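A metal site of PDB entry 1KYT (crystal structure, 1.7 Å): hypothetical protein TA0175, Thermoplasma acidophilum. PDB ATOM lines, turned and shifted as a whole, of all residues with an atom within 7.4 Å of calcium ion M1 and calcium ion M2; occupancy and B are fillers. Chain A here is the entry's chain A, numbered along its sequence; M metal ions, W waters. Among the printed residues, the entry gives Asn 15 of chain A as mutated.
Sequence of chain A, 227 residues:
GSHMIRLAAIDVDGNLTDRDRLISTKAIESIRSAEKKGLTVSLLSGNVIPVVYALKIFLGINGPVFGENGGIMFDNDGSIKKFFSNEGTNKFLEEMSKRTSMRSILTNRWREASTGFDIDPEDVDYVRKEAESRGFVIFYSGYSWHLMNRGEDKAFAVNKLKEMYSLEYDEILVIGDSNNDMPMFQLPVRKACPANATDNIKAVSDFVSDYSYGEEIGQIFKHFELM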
ATOM      1  N   ASP A  11      18.431   9.287   2.015  1.00  0.00           N
ATOM      2  CA  ASP A  11      18.812   9.658   0.655  1.00  0.00           C
ATOM      3  C   ASP A  11      18.199  11.040   0.419  1.00  0.00           C
ATOM      4  O   ASP A  11      16.989  11.182   0.394  1.00  0.00           O
ATOM      5  CB  ASP A  11      18.264   8.611  -0.316  1.00  0.00           C
ATOM      6  CG  ASP A  11      18.212   9.093  -1.764  1.00  0.00           C
ATOM      7  OD1 ASP A  11      18.930  10.025  -2.188  1.00  0.00           O
ATOM      8  OD2 ASP A  11      17.415   8.486  -2.496  1.00  0.00           O
ATOM      9  N   VAL A  12      19.051  12.046   0.270  1.00  0.00           N
ATOM     10  CA  VAL A  12      18.579  13.412   0.083  1.00  0.00           C
ATOM     11  C   VAL A  12      17.695  13.616  -1.152  1.00  0.00           C
ATOM     12  O   VAL A  12      16.527  14.003  -1.015  1.00  0.00           O
ATOM     13  CB  VAL A  12      19.783  14.387   0.016  1.00  0.00           C
ATOM     14  CG1 VAL A  12      19.298  15.816  -0.261  1.00  0.00           C
ATOM     15  CG2 VAL A  12      20.527  14.360   1.337  1.00  0.00           C
ATOM     16  N   ASP A  13      18.225  13.331  -2.320  1.00  0.00           N
ATOM     17  CA  ASP A  13      17.484  13.535  -3.566  1.00  0.00           C
ATOM     18  C   ASP A  13      16.273  12.631  -3.742  1.00  0.00           C
ATOM     19  O   ASP A  13      15.270  13.039  -4.319  1.00  0.00           O
ATOM     20  CB  ASP A  13      18.438  13.412  -4.744  1.00  0.00           C
ATOM     21  CG  ASP A  13      19.695  14.249  -4.542  1.00  0.00           C
ATOM     22  OD1 ASP A  13      20.675  13.729  -3.976  1.00  0.00           O
ATOM     23  OD2 ASP A  13      19.680  15.441  -4.923  1.00  0.00           O
ATOM     24  N   GLY A  14      16.351  11.408  -3.244  1.00  0.00           N
ATOM     25  CA  GLY A  14      15.218  10.528  -3.385  1.00  0.00           C
ATOM     26  C   GLY A  14      14.098  10.775  -2.389  1.00  0.00           C
ATOM     27  O   GLY A  14      12.925  10.601  -2.718  1.00  0.00           O
ATOM     28  N   ASN A  15      14.438  11.217  -1.193  1.00  0.00           N
ATOM     29  CA  ASN A  15      13.386  11.355  -0.191  1.00  0.00           C
ATOM     30  C   ASN A  15      13.100  12.683   0.475  1.00  0.00           C
ATOM     31  O   ASN A  15      12.073  12.832   1.128  1.00  0.00           O
ATOM     32  CB  ASN A  15      13.634  10.313   0.909  1.00  0.00           C
ATOM     33  CG  ASN A  15      13.617   8.895   0.385  1.00  0.00           C
ATOM     34  OD1 ASN A  15      12.569   8.243   0.338  1.00  0.00           O
ATOM     35  ND2 ASN A  15      14.777   8.406  -0.026  1.00  0.00           N
ATOM     36  N   LEU A  16      13.992  13.660   0.340  1.00  0.00           N
ATOM     37  CA  LEU A  16      13.769  14.927   0.999  1.00  0.00           C
ATOM     38  C   LEU A  16      13.280  16.056   0.119  1.00  0.00           C
ATOM     39  O   LEU A  16      13.143  17.188   0.592  1.00  0.00           O
ATOM     40  CB  LEU A  16      15.067  15.363   1.695  1.00  0.00           C
ATOM     41  CG  LEU A  16      15.595  14.401   2.758  1.00  0.00           C
ATOM     42  CD1 LEU A  16      16.845  14.973   3.400  1.00  0.00           C
ATOM     43  CD2 LEU A  16      14.496  14.181   3.805  1.00  0.00           C
ATOM     44  N   THR A  17      12.986  15.748  -1.150  1.00  0.00           N
ATOM     45  CA  THR A  17      12.589  16.792  -2.086  1.00  0.00           C
ATOM     46  C   THR A  17      11.219  16.625  -2.684  1.00  0.00           C
ATOM     47  O   THR A  17      10.637  15.543  -2.622  1.00  0.00           O
ATOM     48  CB  THR A  17      13.605  16.880  -3.271  1.00  0.00           C
ATOM     49  OG1 THR A  17      13.611  15.646  -3.995  1.00  0.00           O
ATOM     50  CG2 THR A  17      15.025  17.132  -2.753  1.00  0.00           C
ATOM     51  N   ASP A  18      10.694  17.687  -3.275  1.00  0.00           N
ATOM     52  CA  ASP A  18       9.378  17.579  -3.885  1.00  0.00           C
ATOM     53  C   ASP A  18       9.490  17.326  -5.374  1.00  0.00           C
ATOM     54  O   ASP A  18      10.583  17.009  -5.877  1.00  0.00           O
ATOM     55  CB  ASP A  18       8.516  18.823  -3.591  1.00  0.00           C
ATOM     56  CG  ASP A  18       9.093  20.114  -4.151  1.00  0.00           C
ATOM     57  OD1 ASP A  18       9.845  20.066  -5.142  1.00  0.00           O
ATOM     58  OD2 ASP A  18       8.762  21.191  -3.610  1.00  0.00           O
ATOM     59  N   TYR A 140      22.165   6.816 -12.407  1.00  0.00           N
ATOM     60  CA  TYR A 140      21.640   8.157 -12.297  1.00  0.00           C
ATOM     61  C   TYR A 140      21.084   8.410 -10.906  1.00  0.00           C
ATOM     62  O   TYR A 140      20.582   7.498 -10.259  1.00  0.00           O
ATOM     63  CB  TYR A 140      20.536   8.367 -13.330  1.00  0.00           C
ATOM     64  CG  TYR A 140      20.065   9.803 -13.397  1.00  0.00           C
ATOM     65  CD1 TYR A 140      19.111  10.295 -12.492  1.00  0.00           C
ATOM     66  CD2 TYR A 140      20.623  10.684 -14.313  1.00  0.00           C
ATOM     67  CE1 TYR A 140      18.741  11.645 -12.516  1.00  0.00           C
ATOM     68  CE2 TYR A 140      20.252  12.024 -14.336  1.00  0.00           C
ATOM     69  CZ  TYR A 140      19.338  12.505 -13.441  1.00  0.00           C
ATOM     70  OH  TYR A 140      19.035  13.836 -13.466  1.00  0.00           O
ATOM     71  N   SER A 141      21.205   9.643 -10.448  1.00  0.00           N
ATOM     72  CA  SER A 141      20.667  10.048  -9.159  1.00  0.00           C
ATOM     73  C   SER A 141      20.697  11.574  -9.031  1.00  0.00           C
ATOM     74  O   SER A 141      21.703  12.205  -9.349  1.00  0.00           O
ATOM     75  CB  SER A 141      21.445   9.404  -8.022  1.00  0.00           C
ATOM     76  OG  SER A 141      20.878   9.735  -6.779  1.00  0.00           O
ATOM     77  N   GLY A 142      19.593  12.146  -8.589  1.00  0.00           N
ATOM     78  CA  GLY A 142      19.562  13.585  -8.420  1.00  0.00           C
ATOM     79  C   GLY A 142      19.611  14.403  -9.690  1.00  0.00           C
ATOM     80  O   GLY A 142      18.658  14.413 -10.479  1.00  0.00           O
ATOM     81  N   LYS A 154      26.114   3.516  -1.164  1.00  0.00           N
ATOM     82  CA  LYS A 154      25.435   3.757   0.090  1.00  0.00           C
ATOM     83  C   LYS A 154      25.678   2.693   1.161  1.00  0.00           C
ATOM     84  O   LYS A 154      25.637   2.983   2.365  1.00  0.00           O
ATOM     85  CB  LYS A 154      23.934   3.929  -0.153  1.00  0.00           C
ATOM     86  CG  LYS A 154      23.562   5.152  -0.993  1.00  0.00           C
ATOM     87  CD  LYS A 154      22.073   5.456  -0.853  1.00  0.00           C
ATOM     88  CE  LYS A 154      21.668   6.672  -1.650  1.00  0.00           C
ATOM     89  NZ  LYS A 154      21.656   6.460  -3.119  1.00  0.00           N
ATOM     90  N   ILE A 175      16.355   5.210   4.778  1.00  0.00           N
ATOM     91  CA  ILE A 175      15.239   5.711   3.991  1.00  0.00           C
ATOM     92  C   ILE A 175      15.734   5.966   2.555  1.00  0.00           C
ATOM     93  O   ILE A 175      16.672   6.735   2.333  1.00  0.00           O
ATOM     94  CB  ILE A 175      14.634   6.984   4.622  1.00  0.00           C
ATOM     95  CG1 ILE A 175      14.161   6.668   6.040  1.00  0.00           C
ATOM     96  CG2 ILE A 175      13.473   7.511   3.790  1.00  0.00           C
ATOM     97  CD1 ILE A 175      13.740   7.878   6.861  1.00  0.00           C
ATOM     98  N   GLY A 176      15.088   5.302   1.606  1.00  0.00           N
ATOM     99  CA  GLY A 176      15.442   5.429   0.214  1.00  0.00           C
ATOM    100  C   GLY A 176      14.229   5.328  -0.684  1.00  0.00           C
ATOM    101  O   GLY A 176      13.082   5.300  -0.213  1.00  0.00           O
ATOM    102  N   ASP A 177      14.439   5.241  -1.989  1.00  0.00           N
ATOM    103  CA  ASP A 177      13.303   5.183  -2.854  1.00  0.00           C
ATOM    104  C   ASP A 177      13.432   4.357  -4.108  1.00  0.00           C
ATOM    105  O   ASP A 177      12.426   4.012  -4.699  1.00  0.00           O
ATOM    106  CB  ASP A 177      12.882   6.615  -3.224  1.00  0.00           C
ATOM    107  CG  ASP A 177      13.893   7.299  -4.112  1.00  0.00           C
ATOM    108  OD1 ASP A 177      15.079   6.973  -4.013  1.00  0.00           O
ATOM    109  OD2 ASP A 177      13.511   8.185  -4.906  1.00  0.00           O
ATOM    110  N   SER A 178      14.649   4.047  -4.532  1.00  0.00           N
ATOM    111  CA  SER A 178      14.819   3.295  -5.757  1.00  0.00           C
ATOM    112  C   SER A 178      15.997   2.325  -5.792  1.00  0.00           C
ATOM    113  O   SER A 178      16.617   2.022  -4.757  1.00  0.00           O
ATOM    114  CB  SER A 178      14.921   4.270  -6.943  1.00  0.00           C
ATOM    115  OG  SER A 178      15.932   5.238  -6.718  1.00  0.00           O
ATOM    116  N   ASN A 179      16.328   1.865  -6.995  1.00  0.00           N
ATOM    117  CA  ASN A 179      17.379   0.885  -7.153  1.00  0.00           C
ATOM    118  C   ASN A 179      18.742   1.382  -6.694  1.00  0.00           C
ATOM    119  O   ASN A 179      19.533   0.597  -6.161  1.00  0.00           O
ATOM    120  CB  ASN A 179      17.441   0.404  -8.594  1.00  0.00           C
ATOM    121  CG  ASN A 179      18.639  -0.465  -8.867  1.00  0.00           C
ATOM    122  OD1 ASN A 179      19.690   0.020  -9.256  1.00  0.00           O
ATOM    123  ND2 ASN A 179      18.494  -1.772  -8.640  1.00  0.00           N
ATOM    124  N   ASN A 180      19.019   2.663  -6.867  1.00  0.00           N
ATOM    125  CA  ASN A 180      20.321   3.156  -6.454  1.00  0.00           C
ATOM    126  C   ASN A 180      20.408   3.233  -4.924  1.00  0.00           C
ATOM    127  O   ASN A 180      21.420   3.664  -4.390  1.00  0.00           O
ATOM    128  CB  ASN A 180      20.647   4.507  -7.120  1.00  0.00           C
ATOM    129  CG  ASN A 180      19.629   5.570  -6.826  1.00  0.00           C
ATOM    130  OD1 ASN A 180      19.005   5.534  -5.762  1.00  0.00           O
ATOM    131  ND2 ASN A 180      19.443   6.516  -7.746  1.00  0.00           N
ATOM    132  N   ASP A 181      19.343   2.813  -4.235  1.00  0.00           N
ATOM    133  CA  ASP A 181      19.350   2.754  -2.775  1.00  0.00           C
ATOM    134  C   ASP A 181      19.399   1.285  -2.331  1.00  0.00           C
ATOM    135  O   ASP A 181      19.539   0.994  -1.132  1.00  0.00           O
ATOM    136  CB  ASP A 181      18.096   3.359  -2.171  1.00  0.00           C
ATOM    137  CG  ASP A 181      17.921   4.793  -2.530  1.00  0.00           C
ATOM    138  OD1 ASP A 181      18.844   5.593  -2.265  1.00  0.00           O
ATOM    139  OD2 ASP A 181      16.839   5.113  -3.079  1.00  0.00           O
ATOM    140  N   MET A 182      19.282   0.363  -3.278  1.00  0.00           N
ATOM    141  CA  MET A 182      19.276  -1.048  -2.877  1.00  0.00           C
ATOM    142  C   MET A 182      20.537  -1.471  -2.122  1.00  0.00           C
ATOM    143  O   MET A 182      20.458  -2.289  -1.214  1.00  0.00           O
ATOM    144  CB  MET A 182      19.026  -1.963  -4.084  1.00  0.00           C
ATOM    145  CG  MET A 182      18.822  -3.437  -3.705  1.00  0.00           C
ATOM    146  SD  MET A 182      17.400  -3.817  -2.383  1.00  0.00           S
ATOM    147  CE  MET A 182      15.921  -3.917  -3.616  1.00  0.00           C
ATOM    148  N   MET A 184      22.056  -0.142   0.247  1.00  0.00           N
ATOM    149  CA  MET A 184      21.887  -0.014   1.686  1.00  0.00           C
ATOM    150  C   MET A 184      20.616  -0.713   2.169  1.00  0.00           C
ATOM    151  O   MET A 184      20.504  -1.027   3.350  1.00  0.00           O
ATOM    152  CB  MET A 184      21.914   1.469   2.141  1.00  0.00           C
ATOM    153  CG  MET A 184      20.808   2.387   1.669  1.00  0.00           C
ATOM    154  SD  MET A 184      20.934   4.127   2.552  1.00  0.00           S
ATOM    155  CE  MET A 184      19.477   5.017   1.636  1.00  0.00           C
ATOM    156  N   PRO A 194       8.969   5.677   0.722  1.00  0.00           N
ATOM    157  CA  PRO A 194       7.775   6.466   0.390  1.00  0.00           C
ATOM    158  C   PRO A 194       6.767   5.697  -0.462  1.00  0.00           C
ATOM    159  O   PRO A 194       7.064   4.594  -0.958  1.00  0.00           O
ATOM    160  CB  PRO A 194       8.363   7.674  -0.329  1.00  0.00           C
ATOM    161  CG  PRO A 194       9.543   7.065  -1.086  1.00  0.00           C
ATOM    162  CD  PRO A 194      10.157   6.154  -0.018  1.00  0.00           C
ATOM    163  N   ASN A 196       5.796   6.281  -3.405  1.00  0.00           N
ATOM    164  CA  ASN A 196       6.195   6.147  -4.799  1.00  0.00           C
ATOM    165  C   ASN A 196       7.527   5.428  -4.965  1.00  0.00           C
ATOM    166  O   ASN A 196       8.188   5.557  -5.990  1.00  0.00           O
ATOM    167  CB  ASN A 196       6.220   7.534  -5.495  1.00  0.00           C
ATOM    168  CG  ASN A 196       7.393   8.410  -5.055  1.00  0.00           C
ATOM    169  OD1 ASN A 196       7.979   8.211  -3.986  1.00  0.00           O
ATOM    170  ND2 ASN A 196       7.744   9.388  -5.875  1.00  0.00           N
ATOM    171  N   ALA A 197       7.932   4.651  -3.953  1.00  0.00           N
ATOM    172  CA  ALA A 197       9.195   3.935  -4.080  1.00  0.00           C
ATOM    173  C   ALA A 197       8.975   2.752  -5.028  1.00  0.00           C
ATOM    174  O   ALA A 197       7.839   2.317  -5.228  1.00  0.00           O
ATOM    175  CB  ALA A 197       9.659   3.447  -2.735  1.00  0.00           C
ATOM    176  N   SER A 212       4.888  10.737   0.052  1.00  0.00           N
ATOM    177  CA  SER A 212       6.105  10.827  -0.751  1.00  0.00           C
ATOM    178  C   SER A 212       6.557  12.300  -0.809  1.00  0.00           C
ATOM    179  O   SER A 212       5.938  13.161  -0.192  1.00  0.00           O
ATOM    180  CB  SER A 212       5.849  10.376  -2.189  1.00  0.00           C
ATOM    181  OG  SER A 212       5.365   9.054  -2.242  1.00  0.00           O
ATOM    182  N   TYR A 213       7.605  12.573  -1.579  1.00  0.00           N
ATOM    183  CA  TYR A 213       8.079  13.948  -1.733  1.00  0.00           C
ATOM    184  C   TYR A 213       8.391  14.679  -0.442  1.00  0.00           C
ATOM    185  O   TYR A 213       8.170  15.881  -0.330  1.00  0.00           O
ATOM    186  CB  TYR A 213       7.048  14.758  -2.535  1.00  0.00           C
ATOM    187  CG  TYR A 213       6.961  14.327  -3.978  1.00  0.00           C
ATOM    188  CD1 TYR A 213       8.097  14.356  -4.799  1.00  0.00           C
ATOM    189  CD2 TYR A 213       5.769  13.854  -4.523  1.00  0.00           C
ATOM    190  CE1 TYR A 213       8.043  13.934  -6.123  1.00  0.00           C
ATOM    191  CE2 TYR A 213       5.702  13.423  -5.850  1.00  0.00           C
ATOM    192  CZ  TYR A 213       6.843  13.464  -6.641  1.00  0.00           C
ATOM    193  OH  TYR A 213       6.785  13.043  -7.951  1.00  0.00           O
ATOM    194  N   GLU A 216       6.900  11.583   3.714  1.00  0.00           N
ATOM    195  CA  GLU A 216       7.030  10.236   4.274  1.00  0.00           C
ATOM    196  C   GLU A 216       7.937  10.275   5.533  1.00  0.00           C
ATOM    197  O   GLU A 216       7.852   9.402   6.391  1.00  0.00           O
ATOM    198  CB  GLU A 216       7.639   9.270   3.236  1.00  0.00           C
ATOM    199  CG  GLU A 216       9.119   9.522   2.915  1.00  0.00           C
ATOM    200  CD  GLU A 216       9.335  10.374   1.675  1.00  0.00           C
ATOM    201  OE1 GLU A 216       8.638  11.402   1.540  1.00  0.00           O
ATOM    202  OE2 GLU A 216      10.207  10.028   0.839  1.00  0.00           O
HETATM  203 CA    CA M   1      17.459   6.961  -4.549  1.00  0.00          CA
HETATM  204 CA    CA M   2      12.022  10.108  -5.089  1.00  0.00          CA
HETATM  205  O   HOH W   1      17.511   8.475  -6.627  1.00  0.00           O
HETATM  206  O   HOH W   2      10.144  11.381  -6.193  1.00  0.00           O
HETATM  207  O   HOH W   3      10.979   8.306  -6.545  1.00  0.00           O
HETATM  208  O   HOH W   4      13.396  10.697  -7.275  1.00  0.00           O
HETATM  209  O   HOH W   5      12.588  12.608  -4.747  1.00  0.00           O
HETATM  210  O   HOH W   6      10.294   9.153  -3.432  1.00  0.00           O
HETATM  211  O   HOH W   7      19.768   8.416  -4.334  1.00  0.00           O
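The side-chain carboxylate (OD2) of Asp 177 binds calcium ion M2 (2.4 Å). Water W2 binds calcium ion M2 (2.5 Å). Calcium ion M2 is bound by water W3, at 2.5 Å. Water W6 is bound to calcium ion M2 (2.6 Å). Calcium ion M2 is bound by the backbone carbonyl oxygen (O) of Gly 14, at 2.6 Å. Calcium ion M2 is bound by water W5 (2.6 Å). Calcium ion M2 is bound by water W4, 2.6 Å away. Calcium ion M2 has seven donor atoms within binding distance.
The side-chain amide oxygen (OD1) of Asn 180 lies close to the side-chain hydroxyl (OG) of Ser 178 (3.2 Å). The side-chain amino group of Lys 154 is in hydrogen-bond range of the backbone carbonyl oxygen of Asn 180 (3.1 Å). ND2 of Asn 180 sits at hydrogen-bond distance from O of Tyr 140, at 2.9 Å. The side-chain hydroxyl (OG) of Ser 178 lies close to the side-chain carboxylate (OD1) of Asp 177 (3.3 Å). The side-chain carboxylate of Asp 181 lies close to the backbone NH of Ser 178 (2.8 Å). The side-chain carboxylate of Asp 11 lies within hydrogen-bond range of the backbone NH of Gly 14 (3.1 Å). N of Asp 13 is in hydrogen-bond range of OD1 of Asp 11, at 3.4 Å. The backbone carbonyl oxygen of Ile 175 lies within hydrogen-bond range of the backbone NH of Asp 11 (3.1 Å).
Calcium ion M1 is bound by OD1 of Asn 180 (2.4 Å), OD1 of Asp 177 (2.4 Å), OD2 of Asp 181 (2.4 Å), OD2 of Asp 11 (2.6 Å), water W1 (2.6 Å) and water W7 (2.7 Å). Calcium ion M1 has six donor atoms within binding distance. Slightly farther from calcium ion M1 lies the side-chain carboxylate (OD1) of Asp 181 (3.0 Å).
Merely in contact with calcium ion M1: Ser 178 (3.2 Å). Of the 27 residues printed, 5 come within 4 Å of calcium ion M1.
Water W7 lies within hydrogen-bond range of OD1 of Asp 11, NZ of Lys 154 and OG of Ser 141. Water W5 bridges O of Asp 13 (2.7 Å) and OG1 of Thr 17 (3.3 Å).
Two residues have an atom within 4 Å of calcium ion M2: Gly 14 and Asp 177. The nearest printed residue that does not touch calcium ion M2 is Asn 196 (4.4 Å).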
